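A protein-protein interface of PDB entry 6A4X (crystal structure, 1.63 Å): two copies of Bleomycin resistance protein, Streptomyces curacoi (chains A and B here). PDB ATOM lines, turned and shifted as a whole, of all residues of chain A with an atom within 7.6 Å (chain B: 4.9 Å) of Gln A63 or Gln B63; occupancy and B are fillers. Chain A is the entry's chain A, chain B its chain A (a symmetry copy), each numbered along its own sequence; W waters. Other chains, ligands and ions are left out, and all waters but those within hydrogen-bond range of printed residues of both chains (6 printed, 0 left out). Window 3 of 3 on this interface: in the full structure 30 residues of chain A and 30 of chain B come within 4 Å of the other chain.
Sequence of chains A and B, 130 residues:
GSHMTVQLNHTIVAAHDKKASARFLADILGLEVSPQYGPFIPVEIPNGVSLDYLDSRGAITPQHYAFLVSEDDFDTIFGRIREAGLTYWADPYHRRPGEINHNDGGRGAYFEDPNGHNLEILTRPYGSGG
ND1 of His A64 is in hydrogen-bond range of O of Asn A118.
The backbone NH of Gln A63 is in hydrogen-bond range of a ring nitrogen (ND1) of His A117, 3.0 Å away.
The backbone carbonyl oxygen (O) of Asn B118 lies within hydrogen-bond range of the backbone NH (N) of Tyr B65 (3.0 Å).
The backbone NH (N) of Gln B63 sits at hydrogen-bond distance from a ring nitrogen (ND1) of His B117 (2.9 Å).
A ring nitrogen (ND1) of His B64 sits at hydrogen-bond distance from the backbone carbonyl oxygen (O) of Asn B118 (3.0 Å).
The backbone carbonyl oxygen of Gln A63 lies within hydrogen-bond range of the backbone NH of Asn A118.
Ile A12 touches Gln B63, and with the chains exchanged Gln A63 touches Ile B12.
Ile A12 touches His B64, and with the chains exchanged His A64 touches Ile B12.
Thr B61 touches its own counterpart, Thr A61.
Gln B63 touches its own counterpart, Gln A63.
Positions printed for both chains: 12, 61, 62, 63, 64, 65, 117 and 118.
Of the 8 pairs that touch across the chains among the printed residues, 6 have their exchanged pair printed and touching as well.
OG1 of Thr B61 is in hydrogen-bond range of OG1 of Thr A61, 2.6 Å away.
The backbone carbonyl oxygen (O) of His B64 sits at hydrogen-bond distance from the side-chain hydroxyl (OG1) of Thr A11.
CD1 of Tyr B65 touches OG1 of Thr A11, 3.7 Å away.
Ile A12 touches Gln B63.
His B64 touches Ile A12.
Gln A63 touches Ile B12.
CG of Gln A63 touches NE2 of Gln B63 (3.3 Å).
CD2 of His A64 touches CD1 of Ile B12, 3.6 Å away.
Gln A63 touches just these residues of chain B: Ile B12 and Gln B63.
Of the printed residues of chain A, Tyr B65 touches Thr A11.
Printed residues of chain A within 4 Å of Ile B12: Gln A63 (3.6 Å) and His A64 (3.6 Å).
Of the printed residues of chain B, His A64 touches Ile B12 (3.6 Å).
Of the printed residues of chain A, His B64 touches Thr A11 and Ile A12.
Water W4 lies within hydrogen-bond range of O of Ile A12 (2.5 Å), NE2 of Gln B63 (2.8 Å), N of His B64 (3.0 Å) and OG1 of Thr A11 (3.5 Å).
Water W2 lies within hydrogen-bond range of O of Ile B12 (2.5 Å), NE2 of Gln A63 (2.8 Å) and N of His A64 (3.0 Å).
Water W1 lies within hydrogen-bond range of OH of Tyr A65, OG1 of Thr A11, NE2 of Gln B63 and O of Ile A12.
Water W3 lies within hydrogen-bond range of OH of Tyr B65 (2.7 Å), NE2 of Gln A63 (3.0 Å) and O of Ile B12 (3.4 Å).
Water W5 lies within hydrogen-bond range of the backbone NH of Ala A14, the side-chain amide nitrogen of Gln B63 and the backbone carbonyl oxygen of Ile A12.
Water W6 bridges the side-chain amide nitrogen of Gln A63 (3.0 Å) and the backbone carbonyl oxygen of Ile B12 (3.4 Å).
Hydrophobic or aromatic side chains of chain A within 4 Å of the printed part of chain B: Ile A12 and His A64.
Of the 8 printed residues of chain B, 5 touch a printed residue of chain A.
Printed residues of chain B that touch a printed residue of chain A: Ile B12, Thr B61, Gln B63, His B64 and Tyr B65.
Hydrophobic or aromatic side chains of chain B within 4 Å of the printed part of chain A: Ile B12, His B64 and Tyr B65.
Among the printed residues, 8 pairs touch across the chains.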
ATOM      1  N   THR A  11     -12.222  19.011 -26.982  1.00  0.00           N
ATOM      2  CA  THR A  11     -10.839  19.022 -26.525  1.00  0.00           C
ATOM      3  C   THR A  11     -10.214  17.714 -26.983  1.00  0.00           C
ATOM      4  O   THR A  11     -10.920  16.762 -27.315  1.00  0.00           O
ATOM      5  CB  THR A  11     -10.723  19.220 -24.992  1.00  0.00           C
ATOM      6  OG1 THR A  11      -9.345  19.429 -24.636  1.00  0.00           O
ATOM      7  CG2 THR A  11     -11.284  18.022 -24.237  1.00  0.00           C
ATOM      8  N   ILE A  12      -8.883  17.680 -27.059  1.00  0.00           N
ATOM      9  CA  ILE A  12      -8.170  16.486 -27.516  1.00  0.00           C
ATOM     10  C   ILE A  12      -7.686  15.716 -26.296  1.00  0.00           C
ATOM     11  O   ILE A  12      -7.157  16.314 -25.353  1.00  0.00           O
ATOM     12  CB  ILE A  12      -6.998  16.856 -28.443  1.00  0.00           C
ATOM     13  CG1 ILE A  12      -7.546  17.521 -29.702  1.00  0.00           C
ATOM     14  CG2 ILE A  12      -6.191  15.612 -28.826  1.00  0.00           C
ATOM     15  CD1 ILE A  12      -6.449  18.125 -30.594  1.00  0.00           C
ATOM     16  N   VAL A  13      -7.870  14.394 -26.313  1.00  0.00           N
ATOM     17  CA  VAL A  13      -7.419  13.502 -25.242  1.00  0.00           C
ATOM     18  C   VAL A  13      -6.309  12.617 -25.795  1.00  0.00           C
ATOM     19  O   VAL A  13      -6.544  11.780 -26.674  1.00  0.00           O
ATOM     20  CB  VAL A  13      -8.562  12.649 -24.680  1.00  0.00           C
ATOM     21  CG1 VAL A  13      -8.070  11.870 -23.475  1.00  0.00           C
ATOM     22  CG2 VAL A  13      -9.752  13.518 -24.285  1.00  0.00           C
ATOM     23  N   ALA A  14      -5.091  12.788 -25.282  1.00  0.00           N
ATOM     24  CA  ALA A  14      -3.975  11.968 -25.736  1.00  0.00           C
ATOM     25  C   ALA A  14      -4.124  10.540 -25.227  1.00  0.00           C
ATOM     26  O   ALA A  14      -4.471  10.314 -24.062  1.00  0.00           O
ATOM     27  CB  ALA A  14      -2.648  12.560 -25.255  1.00  0.00           C
ATOM     28  N   ILE A  60       2.328  10.769 -21.667  1.00  0.00           N
ATOM     29  CA  ILE A  60       1.015  11.406 -21.680  1.00  0.00           C
ATOM     30  C   ILE A  60       0.838  12.162 -20.376  1.00  0.00           C
ATOM     31  O   ILE A  60       0.788  11.558 -19.298  1.00  0.00           O
ATOM     32  CB  ILE A  60      -0.112  10.383 -21.870  1.00  0.00           C
ATOM     33  CG1 ILE A  60       0.006   9.725 -23.244  1.00  0.00           C
ATOM     34  CG2 ILE A  60      -1.458  11.073 -21.674  1.00  0.00           C
ATOM     35  CD1 ILE A  60      -1.040   8.652 -23.495  1.00  0.00           C
ATOM     36  N   THR A  61       0.724  13.473 -20.471  1.00  0.00           N
ATOM     37  CA  THR A  61       0.416  14.280 -19.301  1.00  0.00           C
ATOM     38  C   THR A  61      -1.022  14.009 -18.868  1.00  0.00           C
ATOM     39  O   THR A  61      -1.952  14.190 -19.672  1.00  0.00           O
ATOM     40  CB  THR A  61       0.634  15.760 -19.625  1.00  0.00           C
ATOM     41  OG1 THR A  61       2.007  15.958 -20.006  1.00  0.00           O
ATOM     42  CG2 THR A  61       0.294  16.654 -18.438  1.00  0.00           C
ATOM     43  N   PRO A  62      -1.257  13.557 -17.637  1.00  0.00           N
ATOM     44  CA  PRO A  62      -2.631  13.254 -17.214  1.00  0.00           C
ATOM     45  C   PRO A  62      -3.466  14.523 -17.150  1.00  0.00           C
ATOM     46  O   PRO A  62      -3.049  15.527 -16.567  1.00  0.00           O
ATOM     47  CB  PRO A  62      -2.448  12.631 -15.826  1.00  0.00           C
ATOM     48  CG  PRO A  62      -1.150  13.202 -15.333  1.00  0.00           C
ATOM     49  CD  PRO A  62      -0.274  13.345 -16.556  1.00  0.00           C
ATOM     50  N   GLN A  63      -4.642  14.479 -17.764  1.00  0.00           N
ATOM     51  CA  GLN A  63      -5.586  15.579 -17.677  1.00  0.00           C
ATOM     52  C   GLN A  63      -6.736  15.169 -16.774  1.00  0.00           C
ATOM     53  O   GLN A  63      -6.845  14.014 -16.372  1.00  0.00           O
ATOM     54  CB  GLN A  63      -6.089  15.975 -19.064  1.00  0.00           C
ATOM     55  CG  GLN A  63      -4.984  16.658 -19.878  1.00  0.00           C
ATOM     56  CD  GLN A  63      -4.455  17.900 -19.161  1.00  0.00           C
ATOM     57  OE1 GLN A  63      -3.488  17.822 -18.394  1.00  0.00           O
ATOM     58  NE2 GLN A  63      -5.067  19.033 -19.400  1.00  0.00           N
ATOM     59  N   HIS A  64      -7.588  16.137 -16.441  1.00  0.00           N
ATOM     60  CA  HIS A  64      -8.687  15.912 -15.504  1.00  0.00           C
ATOM     61  C   HIS A  64      -9.994  16.215 -16.219  1.00  0.00           C
ATOM     62  O   HIS A  64     -10.186  17.330 -16.706  1.00  0.00           O
ATOM     63  CB  HIS A  64      -8.559  16.796 -14.263  1.00  0.00           C
ATOM     64  CG  HIS A  64      -9.644  16.564 -13.248  1.00  0.00           C
ATOM     65  ND1 HIS A  64      -9.874  15.328 -12.688  1.00  0.00           N
ATOM     66  CD2 HIS A  64     -10.569  17.395 -12.713  1.00  0.00           C
ATOM     67  CE1 HIS A  64     -10.886  15.406 -11.841  1.00  0.00           C
ATOM     68  NE2 HIS A  64     -11.326  16.650 -11.834  1.00  0.00           N
ATOM     69  N   TYR A  65     -10.891  15.232 -16.264  1.00  0.00           N
ATOM     70  CA  TYR A  65     -12.190  15.381 -16.910  1.00  0.00           C
ATOM     71  C   TYR A  65     -13.248  14.968 -15.902  1.00  0.00           C
ATOM     72  O   TYR A  65     -13.276  13.810 -15.472  1.00  0.00           O
ATOM     73  CB  TYR A  65     -12.282  14.537 -18.183  1.00  0.00           C
ATOM     74  CG  TYR A  65     -11.160  14.813 -19.164  1.00  0.00           C
ATOM     75  CD1 TYR A  65     -11.100  16.017 -19.851  1.00  0.00           C
ATOM     76  CD2 TYR A  65     -10.146  13.876 -19.380  1.00  0.00           C
ATOM     77  CE1 TYR A  65     -10.065  16.281 -20.742  1.00  0.00           C
ATOM     78  CE2 TYR A  65      -9.106  14.128 -20.264  1.00  0.00           C
ATOM     79  CZ  TYR A  65      -9.075  15.336 -20.949  1.00  0.00           C
ATOM     80  OH  TYR A  65      -8.054  15.615 -21.832  1.00  0.00           O
ATOM     81  N   ALA A  66     -14.104  15.909 -15.526  1.00  0.00           N
ATOM     82  CA  ALA A  66     -15.113  15.677 -14.497  1.00  0.00           C
ATOM     83  C   ALA A  66     -16.495  15.750 -15.116  1.00  0.00           C
ATOM     84  O   ALA A  66     -16.804  16.705 -15.832  1.00  0.00           O
ATOM     85  CB  ALA A  66     -14.999  16.704 -13.381  1.00  0.00           C
ATOM     86  N   PHE A 111     -11.367   8.124 -10.677  1.00  0.00           N
ATOM     87  CA  PHE A 111     -10.732   6.904 -11.163  1.00  0.00           C
ATOM     88  C   PHE A 111      -9.846   7.287 -12.341  1.00  0.00           C
ATOM     89  O   PHE A 111      -9.806   8.448 -12.742  1.00  0.00           O
ATOM     90  CB  PHE A 111     -11.770   5.815 -11.498  1.00  0.00           C
ATOM     91  CG  PHE A 111     -12.756   6.197 -12.564  1.00  0.00           C
ATOM     92  CD1 PHE A 111     -12.665   5.641 -13.829  1.00  0.00           C
ATOM     93  CD2 PHE A 111     -13.789   7.098 -12.307  1.00  0.00           C
ATOM     94  CE1 PHE A 111     -13.571   5.977 -14.816  1.00  0.00           C
ATOM     95  CE2 PHE A 111     -14.697   7.443 -13.308  1.00  0.00           C
ATOM     96  CZ  PHE A 111     -14.587   6.881 -14.558  1.00  0.00           C
ATOM     97  N   ASP A 113      -8.301   6.528 -16.379  1.00  0.00           N
ATOM     98  CA  ASP A 113      -8.481   5.855 -17.671  1.00  0.00           C
ATOM     99  C   ASP A 113      -7.211   5.078 -18.048  1.00  0.00           C
ATOM    100  O   ASP A 113      -6.232   5.096 -17.285  1.00  0.00           O
ATOM    101  CB  ASP A 113      -8.937   6.886 -18.726  1.00  0.00           C
ATOM    102  CG  ASP A 113      -7.816   7.410 -19.627  1.00  0.00           C
ATOM    103  OD1 ASP A 113      -6.672   7.584 -19.163  1.00  0.00           O
ATOM    104  OD2 ASP A 113      -8.099   7.679 -20.825  1.00  0.00           O
ATOM    105  N   ASN A 115      -4.817   5.630 -19.840  1.00  0.00           N
ATOM    106  CA  ASN A 115      -3.649   6.471 -20.020  1.00  0.00           C
ATOM    107  C   ASN A 115      -3.250   7.211 -18.756  1.00  0.00           C
ATOM    108  O   ASN A 115      -2.234   7.906 -18.757  1.00  0.00           O
ATOM    109  CB  ASN A 115      -3.923   7.458 -21.144  1.00  0.00           C
ATOM    110  CG  ASN A 115      -4.525   6.774 -22.343  1.00  0.00           C
ATOM    111  OD1 ASN A 115      -3.826   6.062 -23.061  1.00  0.00           O
ATOM    112  ND2 ASN A 115      -5.836   6.957 -22.553  1.00  0.00           N
ATOM    113  N   GLY A 116      -4.017   7.071 -17.678  1.00  0.00           N
ATOM    114  CA  GLY A 116      -3.768   7.834 -16.480  1.00  0.00           C
ATOM    115  C   GLY A 116      -4.539   9.130 -16.362  1.00  0.00           C
ATOM    116  O   GLY A 116      -4.318   9.873 -15.396  1.00  0.00           O
ATOM    117  N   HIS A 117      -5.426   9.445 -17.300  1.00  0.00           N
ATOM    118  CA  HIS A 117      -6.235  10.639 -17.119  1.00  0.00           C
ATOM    119  C   HIS A 117      -7.113  10.464 -15.898  1.00  0.00           C
ATOM    120  O   HIS A 117      -7.578   9.361 -15.605  1.00  0.00           O
ATOM    121  CB  HIS A 117      -7.083  10.921 -18.355  1.00  0.00           C
ATOM    122  CG  HIS A 117      -6.257  11.232 -19.556  1.00  0.00           C
ATOM    123  ND1 HIS A 117      -5.320  12.241 -19.563  1.00  0.00           N
ATOM    124  CD2 HIS A 117      -6.198  10.649 -20.774  1.00  0.00           C
ATOM    125  CE1 HIS A 117      -4.719  12.272 -20.739  1.00  0.00           C
ATOM    126  NE2 HIS A 117      -5.232  11.315 -21.493  1.00  0.00           N
ATOM    127  N   ASN A 118      -7.294  11.555 -15.163  1.00  0.00           N
ATOM    128  CA  ASN A 118      -8.041  11.535 -13.915  1.00  0.00           C
ATOM    129  C   ASN A 118      -9.498  11.809 -14.239  1.00  0.00           C
ATOM    130  O   ASN A 118      -9.862  12.937 -14.579  1.00  0.00           O
ATOM    131  CB  ASN A 118      -7.491  12.568 -12.944  1.00  0.00           C
ATOM    132  CG  ASN A 118      -6.103  12.227 -12.476  1.00  0.00           C
ATOM    133  OD1 ASN A 118      -5.910  11.240 -11.761  1.00  0.00           O
ATOM    134  ND2 ASN A 118      -5.116  13.034 -12.876  1.00  0.00           N
ATOM    135  N   LEU A 119     -10.326  10.780 -14.129  1.00  0.00           N
ATOM    136  CA  LEU A 119     -11.743  10.923 -14.410  1.00  0.00           C
ATOM    137  C   LEU A 119     -12.494  11.077 -13.097  1.00  0.00           C
ATOM    138  O   LEU A 119     -12.173  10.426 -12.100  1.00  0.00           O
ATOM    139  CB  LEU A 119     -12.270   9.723 -15.197  1.00  0.00           C
ATOM    140  CG  LEU A 119     -11.502   9.408 -16.489  1.00  0.00           C
ATOM    141  CD1 LEU A 119     -12.094   8.202 -17.174  1.00  0.00           C
ATOM    142  CD2 LEU A 119     -11.515  10.614 -17.431  1.00  0.00           C
ATOM    143  N   ILE B  12      -9.258  20.824 -15.984  1.00  0.00           N
ATOM    144  CA  ILE B  12      -8.249  21.693 -15.376  1.00  0.00           C
ATOM    145  C   ILE B  12      -7.322  22.196 -16.473  1.00  0.00           C
ATOM    146  O   ILE B  12      -6.895  21.418 -17.333  1.00  0.00           O
ATOM    147  CB  ILE B  12      -7.463  20.953 -14.278  1.00  0.00           C
ATOM    148  CG1 ILE B  12      -8.417  20.572 -13.150  1.00  0.00           C
ATOM    149  CG2 ILE B  12      -6.338  21.832 -13.727  1.00  0.00           C
ATOM    150  CD1 ILE B  12      -7.779  19.640 -12.106  1.00  0.00           C
ATOM    151  N   THR B  61       2.178  21.060 -20.732  1.00  0.00           N
ATOM    152  CA  THR B  61       1.800  20.382 -21.961  1.00  0.00           C
ATOM    153  C   THR B  61       0.652  21.141 -22.620  1.00  0.00           C
ATOM    154  O   THR B  61      -0.401  21.334 -21.990  1.00  0.00           O
ATOM    155  CB  THR B  61       1.411  18.934 -21.652  1.00  0.00           C
ATOM    156  OG1 THR B  61       2.533  18.265 -21.054  1.00  0.00           O
ATOM    157  CG2 THR B  61       0.974  18.186 -22.908  1.00  0.00           C
ATOM    158  N   PRO B  62       0.807  21.608 -23.859  1.00  0.00           N
ATOM    159  CA  PRO B  62      -0.274  22.374 -24.496  1.00  0.00           C
ATOM    160  C   PRO B  62      -1.487  21.492 -24.740  1.00  0.00           C
ATOM    161  O   PRO B  62      -1.370  20.387 -25.277  1.00  0.00           O
ATOM    162  CB  PRO B  62       0.352  22.844 -25.814  1.00  0.00           C
ATOM    163  CG  PRO B  62       1.419  21.827 -26.100  1.00  0.00           C
ATOM    164  CD  PRO B  62       1.966  21.415 -24.753  1.00  0.00           C
ATOM    165  N   GLN B  63      -2.653  21.978 -24.330  1.00  0.00           N
ATOM    166  CA  GLN B  63      -3.902  21.291 -24.609  1.00  0.00           C
ATOM    167  C   GLN B  63      -4.657  22.061 -25.679  1.00  0.00           C
ATOM    168  O   GLN B  63      -4.271  23.164 -26.057  1.00  0.00           O
ATOM    169  CB  GLN B  63      -4.739  21.149 -23.339  1.00  0.00           C
ATOM    170  CG  GLN B  63      -4.109  20.138 -22.374  1.00  0.00           C
ATOM    171  CD  GLN B  63      -3.953  18.767 -23.031  1.00  0.00           C
ATOM    172  OE1 GLN B  63      -2.909  18.465 -23.622  1.00  0.00           O
ATOM    173  NE2 GLN B  63      -4.964  17.940 -22.933  1.00  0.00           N
ATOM    174  N   HIS B  64      -5.732  21.456 -26.181  1.00  0.00           N
ATOM    175  CA  HIS B  64      -6.502  22.035 -27.281  1.00  0.00           C
ATOM    176  C   HIS B  64      -7.930  22.248 -26.805  1.00  0.00           C
ATOM    177  O   HIS B  64      -8.591  21.293 -26.392  1.00  0.00           O
ATOM    178  CB  HIS B  64      -6.496  21.125 -28.510  1.00  0.00           C
ATOM    179  CG  HIS B  64      -7.237  21.702 -29.685  1.00  0.00           C
ATOM    180  ND1 HIS B  64      -6.907  22.919 -30.236  1.00  0.00           N
ATOM    181  CD2 HIS B  64      -8.297  21.245 -30.394  1.00  0.00           C
ATOM    182  CE1 HIS B  64      -7.721  23.185 -31.243  1.00  0.00           C
ATOM    183  NE2 HIS B  64      -8.574  22.185 -31.362  1.00  0.00           N
ATOM    184  N   TYR B  65      -8.404  23.489 -26.880  1.00  0.00           N
ATOM    185  CA  TYR B  65      -9.758  23.841 -26.466  1.00  0.00           C
ATOM    186  C   TYR B  65     -10.409  24.577 -27.624  1.00  0.00           C
ATOM    187  O   TYR B  65      -9.944  25.652 -28.015  1.00  0.00           O
ATOM    188  CB  TYR B  65      -9.751  24.701 -25.201  1.00  0.00           C
ATOM    189  CG  TYR B  65      -8.986  24.069 -24.054  1.00  0.00           C
ATOM    190  CD1 TYR B  65      -9.482  22.947 -23.405  1.00  0.00           C
ATOM    191  CD2 TYR B  65      -7.753  24.582 -23.642  1.00  0.00           C
ATOM    192  CE1 TYR B  65      -8.777  22.355 -22.362  1.00  0.00           C
ATOM    193  CE2 TYR B  65      -7.039  23.999 -22.604  1.00  0.00           C
ATOM    194  CZ  TYR B  65      -7.562  22.884 -21.962  1.00  0.00           C
ATOM    195  OH  TYR B  65      -6.875  22.283 -20.930  1.00  0.00           O
ATOM    196  N   HIS B 117      -1.472  26.936 -24.760  1.00  0.00           N
ATOM    197  CA  HIS B 117      -2.617  26.111 -25.111  1.00  0.00           C
ATOM    198  C   HIS B 117      -3.154  26.554 -26.456  1.00  0.00           C
ATOM    199  O   HIS B 117      -3.132  27.740 -26.788  1.00  0.00           O
ATOM    200  CB  HIS B 117      -3.703  26.195 -24.045  1.00  0.00           C
ATOM    201  CG  HIS B 117      -3.259  25.643 -22.733  1.00  0.00           C
ATOM    202  ND1 HIS B 117      -2.766  24.365 -22.601  1.00  0.00           N
ATOM    203  CD2 HIS B 117      -3.198  26.204 -21.504  1.00  0.00           C
ATOM    204  CE1 HIS B 117      -2.424  24.156 -21.342  1.00  0.00           C
ATOM    205  NE2 HIS B 117      -2.674  25.257 -20.655  1.00  0.00           N
ATOM    206  N   ASN B 118      -3.591  25.580 -27.246  1.00  0.00           N
ATOM    207  CA  ASN B 118      -4.060  25.829 -28.600  1.00  0.00           C
ATOM    208  C   ASN B 118      -5.549  26.111 -28.533  1.00  0.00           C
ATOM    209  O   ASN B 118      -6.348  25.202 -28.295  1.00  0.00           O
ATOM    210  CB  ASN B 118      -3.766  24.636 -29.497  1.00  0.00           C
ATOM    211  CG  ASN B 118      -2.292  24.437 -29.714  1.00  0.00           C
ATOM    212  OD1 ASN B 118      -1.637  25.264 -30.355  1.00  0.00           O
ATOM    213  ND2 ASN B 118      -1.745  23.341 -29.180  1.00  0.00           N
HETATM  214  O   HOH W   1      -7.892  18.160 -22.596  1.00  0.00           O
HETATM  215  O   HOH W   2      -6.756  18.898 -17.128  1.00  0.00           O
HETATM  216  O   HOH W   3      -7.775  19.876 -20.230  1.00  0.00           O
HETATM  217  O   HOH W   4      -6.083  18.605 -25.452  1.00  0.00           O
HETATM  218  O   HOH W   5      -4.674  14.989 -23.458  1.00  0.00           O
HETATM  219  O   HOH W   6      -3.821  21.694 -18.741  1.00  0.00           O
